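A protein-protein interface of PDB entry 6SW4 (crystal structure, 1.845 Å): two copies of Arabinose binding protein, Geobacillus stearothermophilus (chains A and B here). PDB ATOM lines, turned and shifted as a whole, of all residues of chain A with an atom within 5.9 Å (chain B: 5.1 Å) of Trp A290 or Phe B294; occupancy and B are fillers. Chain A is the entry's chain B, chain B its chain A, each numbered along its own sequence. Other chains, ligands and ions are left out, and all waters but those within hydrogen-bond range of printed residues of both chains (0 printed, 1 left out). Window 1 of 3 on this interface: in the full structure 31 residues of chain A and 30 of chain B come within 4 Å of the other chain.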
ATOM      1  N   GLY A  67     -17.189  22.264  20.952  1.00  0.00           N
ATOM      2  CA  GLY A  67     -16.658  21.409  21.999  1.00  0.00           C
ATOM      3  C   GLY A  67     -17.758  20.774  22.825  1.00  0.00           C
ATOM      4  O   GLY A  67     -17.749  19.565  23.067  1.00  0.00           O
ATOM      5  N   ALA A  71     -18.562  16.713  22.804  1.00  0.00           N
ATOM      6  CA  ALA A  71     -18.596  15.937  24.039  1.00  0.00           C
ATOM      7  C   ALA A  71     -19.945  15.256  24.208  1.00  0.00           C
ATOM      8  O   ALA A  71     -20.011  14.077  24.583  1.00  0.00           O
ATOM      9  CB  ALA A  71     -18.296  16.835  25.240  1.00  0.00           C
ATOM     10  N   LEU A 147     -13.132  26.608  33.812  1.00  0.00           N
ATOM     11  CA  LEU A 147     -12.303  26.188  32.692  1.00  0.00           C
ATOM     12  C   LEU A 147     -12.045  27.404  31.803  1.00  0.00           C
ATOM     13  O   LEU A 147     -12.943  27.845  31.076  1.00  0.00           O
ATOM     14  CB  LEU A 147     -12.974  25.062  31.912  1.00  0.00           C
ATOM     15  CG  LEU A 147     -13.325  23.775  32.674  1.00  0.00           C
ATOM     16  CD1 LEU A 147     -14.749  23.787  33.252  1.00  0.00           C
ATOM     17  CD2 LEU A 147     -13.149  22.562  31.778  1.00  0.00           C
ATOM     18  N   TRP A 285     -12.730  25.573  22.283  1.00  0.00           N
ATOM     19  CA  TRP A 285     -13.238  24.223  22.090  1.00  0.00           C
ATOM     20  C   TRP A 285     -12.985  23.372  23.329  1.00  0.00           C
ATOM     21  O   TRP A 285     -13.859  22.618  23.767  1.00  0.00           O
ATOM     22  CB  TRP A 285     -12.604  23.583  20.864  1.00  0.00           C
ATOM     23  CG  TRP A 285     -13.211  22.258  20.510  1.00  0.00           C
ATOM     24  CD1 TRP A 285     -14.156  22.019  19.551  1.00  0.00           C
ATOM     25  CD2 TRP A 285     -12.902  20.982  21.092  1.00  0.00           C
ATOM     26  NE1 TRP A 285     -14.453  20.676  19.503  1.00  0.00           N
ATOM     27  CE2 TRP A 285     -13.700  20.019  20.438  1.00  0.00           C
ATOM     28  CE3 TRP A 285     -12.034  20.560  22.101  1.00  0.00           C
ATOM     29  CZ2 TRP A 285     -13.647  18.662  20.757  1.00  0.00           C
ATOM     30  CZ3 TRP A 285     -11.985  19.208  22.418  1.00  0.00           C
ATOM     31  CH2 TRP A 285     -12.786  18.276  21.748  1.00  0.00           C
ATOM     32  N   ASN A 286     -11.784  23.487  23.905  1.00  0.00           N
ATOM     33  CA  ASN A 286     -11.485  22.792  25.154  1.00  0.00           C
ATOM     34  C   ASN A 286     -12.449  23.192  26.256  1.00  0.00           C
ATOM     35  O   ASN A 286     -12.884  22.348  27.050  1.00  0.00           O
ATOM     36  CB  ASN A 286     -10.053  23.090  25.586  1.00  0.00           C
ATOM     37  CG  ASN A 286      -9.067  22.211  24.913  1.00  0.00           C
ATOM     38  OD1 ASN A 286      -9.407  21.113  24.440  1.00  0.00           O
ATOM     39  ND2 ASN A 286      -7.815  22.650  24.885  1.00  0.00           N
ATOM     40  N   MET A 287     -12.768  24.480  26.342  1.00  0.00           N
ATOM     41  CA  MET A 287     -13.719  24.946  27.339  1.00  0.00           C
ATOM     42  C   MET A 287     -15.042  24.200  27.245  1.00  0.00           C
ATOM     43  O   MET A 287     -15.608  23.797  28.265  1.00  0.00           O
ATOM     44  CB  MET A 287     -13.951  26.445  27.183  1.00  0.00           C
ATOM     45  CG  MET A 287     -12.714  27.289  27.439  1.00  0.00           C
ATOM     46  SD  MET A 287     -13.117  29.003  27.083  1.00  0.00           S
ATOM     47  CE  MET A 287     -11.521  29.807  27.277  1.00  0.00           C
ATOM     48  N   GLY A 288     -15.570  24.033  26.032  1.00  0.00           N
ATOM     49  CA  GLY A 288     -16.865  23.385  25.903  1.00  0.00           C
ATOM     50  C   GLY A 288     -16.775  21.886  26.100  1.00  0.00           C
ATOM     51  O   GLY A 288     -17.578  21.293  26.831  1.00  0.00           O
ATOM     52  N   TYR A 289     -15.781  21.256  25.473  1.00  0.00           N
ATOM     53  CA  TYR A 289     -15.668  19.810  25.573  1.00  0.00           C
ATOM     54  C   TYR A 289     -15.454  19.372  27.020  1.00  0.00           C
ATOM     55  O   TYR A 289     -16.138  18.467  27.516  1.00  0.00           O
ATOM     56  CB  TYR A 289     -14.547  19.304  24.677  1.00  0.00           C
ATOM     57  CG  TYR A 289     -14.476  17.800  24.695  1.00  0.00           C
ATOM     58  CD1 TYR A 289     -13.755  17.140  25.672  1.00  0.00           C
ATOM     59  CD2 TYR A 289     -15.152  17.041  23.752  1.00  0.00           C
ATOM     60  CE1 TYR A 289     -13.685  15.786  25.709  1.00  0.00           C
ATOM     61  CE2 TYR A 289     -15.091  15.667  23.783  1.00  0.00           C
ATOM     62  CZ  TYR A 289     -14.362  15.047  24.769  1.00  0.00           C
ATOM     63  OH  TYR A 289     -14.284  13.688  24.824  1.00  0.00           O
ATOM     64  N   TRP A 290     -14.518  20.009  27.724  1.00  0.00           N
ATOM     65  CA  TRP A 290     -14.232  19.542  29.075  1.00  0.00           C
ATOM     66  C   TRP A 290     -15.237  20.071  30.090  1.00  0.00           C
ATOM     67  O   TRP A 290     -15.474  19.405  31.104  1.00  0.00           O
ATOM     68  CB  TRP A 290     -12.781  19.883  29.426  1.00  0.00           C
ATOM     69  CG  TRP A 290     -11.869  19.035  28.588  1.00  0.00           C
ATOM     70  CD1 TRP A 290     -11.149  19.437  27.500  1.00  0.00           C
ATOM     71  CD2 TRP A 290     -11.634  17.631  28.725  1.00  0.00           C
ATOM     72  NE1 TRP A 290     -10.456  18.381  26.979  1.00  0.00           N
ATOM     73  CE2 TRP A 290     -10.750  17.255  27.705  1.00  0.00           C
ATOM     74  CE3 TRP A 290     -12.086  16.652  29.622  1.00  0.00           C
ATOM     75  CZ2 TRP A 290     -10.301  15.945  27.553  1.00  0.00           C
ATOM     76  CZ3 TRP A 290     -11.634  15.364  29.478  1.00  0.00           C
ATOM     77  CH2 TRP A 290     -10.755  15.014  28.454  1.00  0.00           C
ATOM     78  N   SER A 291     -15.877  21.220  29.825  1.00  0.00           N
ATOM     79  CA  SER A 291     -17.024  21.618  30.638  1.00  0.00           C
ATOM     80  C   SER A 291     -18.074  20.517  30.706  1.00  0.00           C
ATOM     81  O   SER A 291     -18.630  20.240  31.775  1.00  0.00           O
ATOM     82  CB  SER A 291     -17.679  22.874  30.083  1.00  0.00           C
ATOM     83  OG  SER A 291     -17.129  24.000  30.716  1.00  0.00           O
ATOM     84  N   LEU A 292     -18.383  19.905  29.557  1.00  0.00           N
ATOM     85  CA  LEU A 292     -19.432  18.890  29.531  1.00  0.00           C
ATOM     86  C   LEU A 292     -18.948  17.592  30.160  1.00  0.00           C
ATOM     87  O   LEU A 292     -19.714  16.916  30.856  1.00  0.00           O
ATOM     88  CB  LEU A 292     -19.914  18.644  28.099  1.00  0.00           C
ATOM     89  CG  LEU A 292     -21.125  17.701  27.986  1.00  0.00           C
ATOM     90  CD1 LEU A 292     -22.275  18.136  28.879  1.00  0.00           C
ATOM     91  CD2 LEU A 292     -21.592  17.601  26.578  1.00  0.00           C
ATOM     92  N   GLN A 293     -17.677  17.231  29.939  1.00  0.00           N
ATOM     93  CA  GLN A 293     -17.131  16.091  30.662  1.00  0.00           C
ATOM     94  C   GLN A 293     -17.315  16.278  32.157  1.00  0.00           C
ATOM     95  O   GLN A 293     -17.726  15.349  32.863  1.00  0.00           O
ATOM     96  CB  GLN A 293     -15.660  15.897  30.322  1.00  0.00           C
ATOM     97  CG  GLN A 293     -15.441  15.544  28.894  1.00  0.00           C
ATOM     98  CD  GLN A 293     -15.932  14.141  28.560  1.00  0.00           C
ATOM     99  OE1 GLN A 293     -16.129  13.301  29.446  1.00  0.00           O
ATOM    100  NE2 GLN A 293     -16.147  13.889  27.270  1.00  0.00           N
ATOM    101  N   PHE A 294     -17.062  17.498  32.646  1.00  0.00           N
ATOM    102  CA  PHE A 294     -17.149  17.770  34.076  1.00  0.00           C
ATOM    103  C   PHE A 294     -18.599  17.726  34.561  1.00  0.00           C
ATOM    104  O   PHE A 294     -18.884  17.173  35.628  1.00  0.00           O
ATOM    105  CB  PHE A 294     -16.516  19.130  34.391  1.00  0.00           C
ATOM    106  CG  PHE A 294     -15.003  19.089  34.592  1.00  0.00           C
ATOM    107  CD1 PHE A 294     -14.252  17.987  34.222  1.00  0.00           C
ATOM    108  CD2 PHE A 294     -14.353  20.162  35.174  1.00  0.00           C
ATOM    109  CE1 PHE A 294     -12.870  17.939  34.427  1.00  0.00           C
ATOM    110  CE2 PHE A 294     -12.961  20.139  35.381  1.00  0.00           C
ATOM    111  CZ  PHE A 294     -12.226  19.038  35.001  1.00  0.00           C
ATOM    112  N   LEU A 295     -19.524  18.304  33.797  1.00  0.00           N
ATOM    113  CA  LEU A 295     -20.930  18.223  34.175  1.00  0.00           C
ATOM    114  C   LEU A 295     -21.426  16.790  34.134  1.00  0.00           C
ATOM    115  O   LEU A 295     -22.231  16.382  34.980  1.00  0.00           O
ATOM    116  CB  LEU A 295     -21.773  19.097  33.260  1.00  0.00           C
ATOM    117  CG  LEU A 295     -21.459  20.583  33.374  1.00  0.00           C
ATOM    118  CD1 LEU A 295     -21.990  21.282  32.141  1.00  0.00           C
ATOM    119  CD2 LEU A 295     -22.034  21.163  34.651  1.00  0.00           C
ATOM    120  N   VAL A 317      -9.237  24.398  35.191  1.00  0.00           N
ATOM    121  CA  VAL A 317      -8.682  23.784  34.010  1.00  0.00           C
ATOM    122  C   VAL A 317      -8.178  24.903  33.131  1.00  0.00           C
ATOM    123  O   VAL A 317      -8.970  25.726  32.671  1.00  0.00           O
ATOM    124  CB  VAL A 317      -9.736  22.953  33.270  1.00  0.00           C
ATOM    125  CG1 VAL A 317      -9.159  22.425  31.978  1.00  0.00           C
ATOM    126  CG2 VAL A 317     -10.192  21.792  34.175  1.00  0.00           C
ATOM    127  N   VAL B 132       1.017  12.507  29.624  1.00  0.00           N
ATOM    128  CA  VAL B 132       0.634  13.613  30.493  1.00  0.00           C
ATOM    129  C   VAL B 132       1.462  13.502  31.760  1.00  0.00           C
ATOM    130  O   VAL B 132       1.908  12.419  32.153  1.00  0.00           O
ATOM    131  CB  VAL B 132      -0.879  13.659  30.819  1.00  0.00           C
ATOM    132  CG1 VAL B 132      -1.729  13.806  29.537  1.00  0.00           C
ATOM    133  CG2 VAL B 132      -1.302  12.448  31.659  1.00  0.00           C
ATOM    134  N   SER B 145      -0.028  17.776  28.956  1.00  0.00           N
ATOM    135  CA  SER B 145      -0.776  18.342  30.066  1.00  0.00           C
ATOM    136  C   SER B 145      -0.015  18.082  31.355  1.00  0.00           C
ATOM    137  O   SER B 145       0.811  17.175  31.423  1.00  0.00           O
ATOM    138  CB  SER B 145      -2.184  17.754  30.177  1.00  0.00           C
ATOM    139  OG  SER B 145      -3.044  18.616  30.911  1.00  0.00           O
ATOM    140  N   LEU B 147      -1.247  17.704  35.497  1.00  0.00           N
ATOM    141  CA  LEU B 147      -2.396  17.645  36.388  1.00  0.00           C
ATOM    142  C   LEU B 147      -1.835  17.574  37.788  1.00  0.00           C
ATOM    143  O   LEU B 147      -1.229  16.574  38.152  1.00  0.00           O
ATOM    144  CB  LEU B 147      -3.274  16.426  36.112  1.00  0.00           C
ATOM    145  CG  LEU B 147      -3.888  16.464  34.719  1.00  0.00           C
ATOM    146  CD1 LEU B 147      -3.026  15.690  33.740  1.00  0.00           C
ATOM    147  CD2 LEU B 147      -5.286  15.868  34.835  1.00  0.00           C
ATOM    148  N   TRP B 290      -8.090  12.019  36.112  1.00  0.00           N
ATOM    149  CA  TRP B 290      -8.110  12.842  34.915  1.00  0.00           C
ATOM    150  C   TRP B 290      -6.874  12.635  34.041  1.00  0.00           C
ATOM    151  O   TRP B 290      -6.959  12.887  32.835  1.00  0.00           O
ATOM    152  CB  TRP B 290      -8.339  14.307  35.293  1.00  0.00           C
ATOM    153  CG  TRP B 290      -9.717  14.481  35.843  1.00  0.00           C
ATOM    154  CD1 TRP B 290     -10.075  14.619  37.161  1.00  0.00           C
ATOM    155  CD2 TRP B 290     -10.931  14.457  35.102  1.00  0.00           C
ATOM    156  NE1 TRP B 290     -11.439  14.710  37.274  1.00  0.00           N
ATOM    157  CE2 TRP B 290     -11.989  14.621  36.023  1.00  0.00           C
ATOM    158  CE3 TRP B 290     -11.230  14.322  33.745  1.00  0.00           C
ATOM    159  CZ2 TRP B 290     -13.333  14.633  35.625  1.00  0.00           C
ATOM    160  CZ3 TRP B 290     -12.558  14.331  33.358  1.00  0.00           C
ATOM    161  CH2 TRP B 290     -13.587  14.498  34.294  1.00  0.00           C
ATOM    162  N   SER B 291      -5.761  12.126  34.584  1.00  0.00           N
ATOM    163  CA  SER B 291      -4.649  11.721  33.721  1.00  0.00           C
ATOM    164  C   SER B 291      -5.102  10.653  32.737  1.00  0.00           C
ATOM    165  O   SER B 291      -4.849  10.758  31.535  1.00  0.00           O
ATOM    166  CB  SER B 291      -3.454  11.202  34.523  1.00  0.00           C
ATOM    167  OG  SER B 291      -2.745  12.251  35.167  1.00  0.00           O
ATOM    168  N   LEU B 292      -5.801   9.624  33.230  1.00  0.00           N
ATOM    169  CA  LEU B 292      -6.250   8.580  32.312  1.00  0.00           C
ATOM    170  C   LEU B 292      -7.302   9.114  31.358  1.00  0.00           C
ATOM    171  O   LEU B 292      -7.266   8.794  30.169  1.00  0.00           O
ATOM    172  CB  LEU B 292      -6.790   7.372  33.072  1.00  0.00           C
ATOM    173  CG  LEU B 292      -6.591   6.020  32.347  1.00  0.00           C
ATOM    174  CD1 LEU B 292      -7.091   4.887  33.182  1.00  0.00           C
ATOM    175  CD2 LEU B 292      -7.272   5.964  31.056  1.00  0.00           C
ATOM    176  N   GLN B 293      -8.240   9.921  31.857  1.00  0.00           N
ATOM    177  CA  GLN B 293      -9.261  10.521  31.006  1.00  0.00           C
ATOM    178  C   GLN B 293      -8.638  11.311  29.864  1.00  0.00           C
ATOM    179  O   GLN B 293      -9.060  11.211  28.700  1.00  0.00           O
ATOM    180  CB  GLN B 293     -10.169  11.424  31.832  1.00  0.00           C
ATOM    181  CG  GLN B 293     -11.066  10.682  32.789  1.00  0.00           C
ATOM    182  CD  GLN B 293     -12.254  10.054  32.072  1.00  0.00           C
ATOM    183  OE1 GLN B 293     -13.392  10.529  32.173  1.00  0.00           O
ATOM    184  NE2 GLN B 293     -11.988   9.013  31.323  1.00  0.00           N
ATOM    185  N   PHE B 294      -7.624  12.110  30.182  1.00  0.00           N
ATOM    186  CA  PHE B 294      -6.918  12.849  29.145  1.00  0.00           C
ATOM    187  C   PHE B 294      -6.155  11.908  28.213  1.00  0.00           C
ATOM    188  O   PHE B 294      -6.167  12.080  26.992  1.00  0.00           O
ATOM    189  CB  PHE B 294      -5.962  13.862  29.799  1.00  0.00           C
ATOM    190  CG  PHE B 294      -6.614  15.155  30.211  1.00  0.00           C
ATOM    191  CD1 PHE B 294      -7.988  15.285  30.310  1.00  0.00           C
ATOM    192  CD2 PHE B 294      -5.817  16.266  30.476  1.00  0.00           C
ATOM    193  CE1 PHE B 294      -8.560  16.480  30.678  1.00  0.00           C
ATOM    194  CE2 PHE B 294      -6.371  17.482  30.834  1.00  0.00           C
ATOM    195  CZ  PHE B 294      -7.747  17.605  30.942  1.00  0.00           C
ATOM    196  N   LEU B 295      -5.460  10.915  28.769  1.00  0.00           N
ATOM    197  CA  LEU B 295      -4.692  10.003  27.928  1.00  0.00           C
ATOM    198  C   LEU B 295      -5.616   9.219  27.005  1.00  0.00           C
ATOM    199  O   LEU B 295      -5.385   9.138  25.791  1.00  0.00           O
ATOM    200  CB  LEU B 295      -3.883   9.046  28.791  1.00  0.00           C
ATOM    201  CG  LEU B 295      -2.651   9.618  29.467  1.00  0.00           C
ATOM    202  CD1 LEU B 295      -2.068   8.573  30.425  1.00  0.00           C
ATOM    203  CD2 LEU B 295      -1.631  10.102  28.439  1.00  0.00           C
ATOM    204  N   PHE B 296      -6.666   8.623  27.575  1.00  0.00           N
ATOM    205  CA  PHE B 296      -7.645   7.903  26.770  1.00  0.00           C
ATOM    206  C   PHE B 296      -8.148   8.789  25.650  1.00  0.00           C
ATOM    207  O   PHE B 296      -8.307   8.344  24.507  1.00  0.00           O
ATOM    208  CB  PHE B 296      -8.801   7.437  27.660  1.00  0.00           C
ATOM    209  CG  PHE B 296      -9.972   6.852  26.906  1.00  0.00           C
ATOM    210  CD1 PHE B 296     -10.982   7.673  26.413  1.00  0.00           C
ATOM    211  CD2 PHE B 296     -10.083   5.478  26.731  1.00  0.00           C
ATOM    212  CE1 PHE B 296     -12.058   7.137  25.736  1.00  0.00           C
ATOM    213  CE2 PHE B 296     -11.168   4.944  26.059  1.00  0.00           C
ATOM    214  CZ  PHE B 296     -12.150   5.790  25.560  1.00  0.00           C
ATOM    215  N   HIS B 297      -8.331  10.069  25.950  1.00  0.00           N
ATOM    216  CA  HIS B 297      -8.903  10.988  24.983  1.00  0.00           C
ATOM    217  C   HIS B 297      -7.950  11.282  23.827  1.00  0.00           C
ATOM    218  O   HIS B 297      -8.396  11.414  22.681  1.00  0.00           O
ATOM    219  CB  HIS B 297      -9.290  12.265  25.699  1.00  0.00           C
ATOM    220  CG  HIS B 297      -9.785  13.328  24.789  1.00  0.00           C
ATOM    221  ND1 HIS B 297     -11.121  13.485  24.501  1.00  0.00           N
ATOM    222  CD2 HIS B 297      -9.131  14.300  24.112  1.00  0.00           C
ATOM    223  CE1 HIS B 297     -11.272  14.507  23.678  1.00  0.00           C
ATOM    224  NE2 HIS B 297     -10.081  15.017  23.427  1.00  0.00           N
ATOM    225  N   LEU B 298      -6.644  11.395  24.097  1.00  0.00           N
ATOM    226  CA  LEU B 298      -5.690  11.640  23.018  1.00  0.00           C
ATOM    227  C   LEU B 298      -5.519  10.401  22.145  1.00  0.00           C
ATOM    228  O   LEU B 298      -5.370  10.510  20.921  1.00  0.00           O
ATOM    229  CB  LEU B 298      -4.341  12.073  23.595  1.00  0.00           C
ATOM    230  CG  LEU B 298      -4.185  13.562  23.921  1.00  0.00           C
ATOM    231  CD1 LEU B 298      -2.744  13.885  24.295  1.00  0.00           C
ATOM    232  CD2 LEU B 298      -4.648  14.431  22.756  1.00  0.00           C
ATOM    233  N   LEU B 313      -5.049  18.900  24.418  1.00  0.00           N
ATOM    234  CA  LEU B 313      -5.462  18.754  25.839  1.00  0.00           C
ATOM    235  C   LEU B 313      -5.324  20.080  26.589  1.00  0.00           C
ATOM    236  O   LEU B 313      -4.442  20.877  26.240  1.00  0.00           O
ATOM    237  CB  LEU B 313      -4.549  17.718  26.500  1.00  0.00           C
ATOM    238  CG  LEU B 313      -4.927  16.256  26.291  1.00  0.00           C
ATOM    239  CD1 LEU B 313      -4.090  15.364  27.187  1.00  0.00           C
ATOM    240  CD2 LEU B 313      -6.407  16.042  26.553  1.00  0.00           C
ATOM    241  N   PRO B 314      -6.131  20.328  27.645  1.00  0.00           N
ATOM    242  CA  PRO B 314      -5.951  21.506  28.500  1.00  0.00           C
ATOM    243  C   PRO B 314      -4.530  21.421  29.085  1.00  0.00           C
ATOM    244  O   PRO B 314      -4.109  20.369  29.521  1.00  0.00           O
ATOM    245  CB  PRO B 314      -7.038  21.344  29.569  1.00  0.00           C
ATOM    246  CG  PRO B 314      -8.096  20.527  28.872  1.00  0.00           C
ATOM    247  CD  PRO B 314      -7.308  19.551  28.025  1.00  0.00           C
ATOM    248  N   VAL B 317      -4.462  21.027  34.847  1.00  0.00           N
ATOM    249  CA  VAL B 317      -5.646  20.714  35.627  1.00  0.00           C
ATOM    250  C   VAL B 317      -5.251  20.848  37.088  1.00  0.00           C
ATOM    251  O   VAL B 317      -4.348  20.143  37.550  1.00  0.00           O
ATOM    252  CB  VAL B 317      -6.168  19.299  35.327  1.00  0.00           C
ATOM    253  CG1 VAL B 317      -7.293  18.944  36.282  1.00  0.00           C
ATOM    254  CG2 VAL B 317      -6.680  19.206  33.882  1.00  0.00           C
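NE2 of Gln A293 lies within hydrogen-bond range of OH of Tyr A289 (3.1 Å).
O of Pro B314 is in hydrogen-bond range of OG of Ser B145 (2.5 Å).
A ring nitrogen (ND1) of His B297 is in hydrogen-bond range of the side-chain hydroxyl of Tyr A289, 3.2 Å away.
Leu B313 touches Asn A286.
Pro B314 touches Asn A286 (N to ND2, 3.98 Å).
Phe B294 touches Trp A290.
CG of His B297 touches CZ2 of Trp A290, at 3.8 Å.
Trp A290 touches Pro B314 (NE1 to CD, 3.5 Å).
CH2 of Trp B290 touches CE1 of Phe A294, at 3.5 Å.
Val A317 touches Pro B314 (CG1 to CB, 3.4 Å).
Printed residues of chain B within 4 Å of Asn A286: Leu B313 and Pro B314.
Met A287 touches none of the printed residues of chain B.
Ser B145 touches none of the printed residues of chain A.
Of the printed residues of chain A, Trp B290 touches Phe A294 (3.5 Å).
Of the printed residues of chain A, His B297 touches Tyr A289 and Trp A290.
Printed residues of chain A within 4 Å of Pro B314: Asn A286 (3.98 Å), Trp A290 (3.5 Å) and Val A317 (3.4 Å).
The nearest printed residue of chain B that does not touch Asn A286 is His B297 (6.2 Å).
Trp A290 touches Phe B294, and with the chains exchanged Phe A294 touches Trp B290.
Printed residues of chain B that touch a printed residue of chain A: Trp B290, Phe B294, His B297, Leu B313 and Pro B314.
Of the 15 printed residues of chain A, 5 touch a printed residue of chain B.
Hydrophobic or aromatic side chains of chain A within 4 Å of the printed part of chain B: Tyr A289, Trp A290, Phe A294 and Val A317.
Among the printed residues, 8 pairs touch across the chains.
Among the printed residues, no Asp or Glu carboxylate lies within 4 Å of a Lys or Arg side-chain nitrogen of the other chain.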
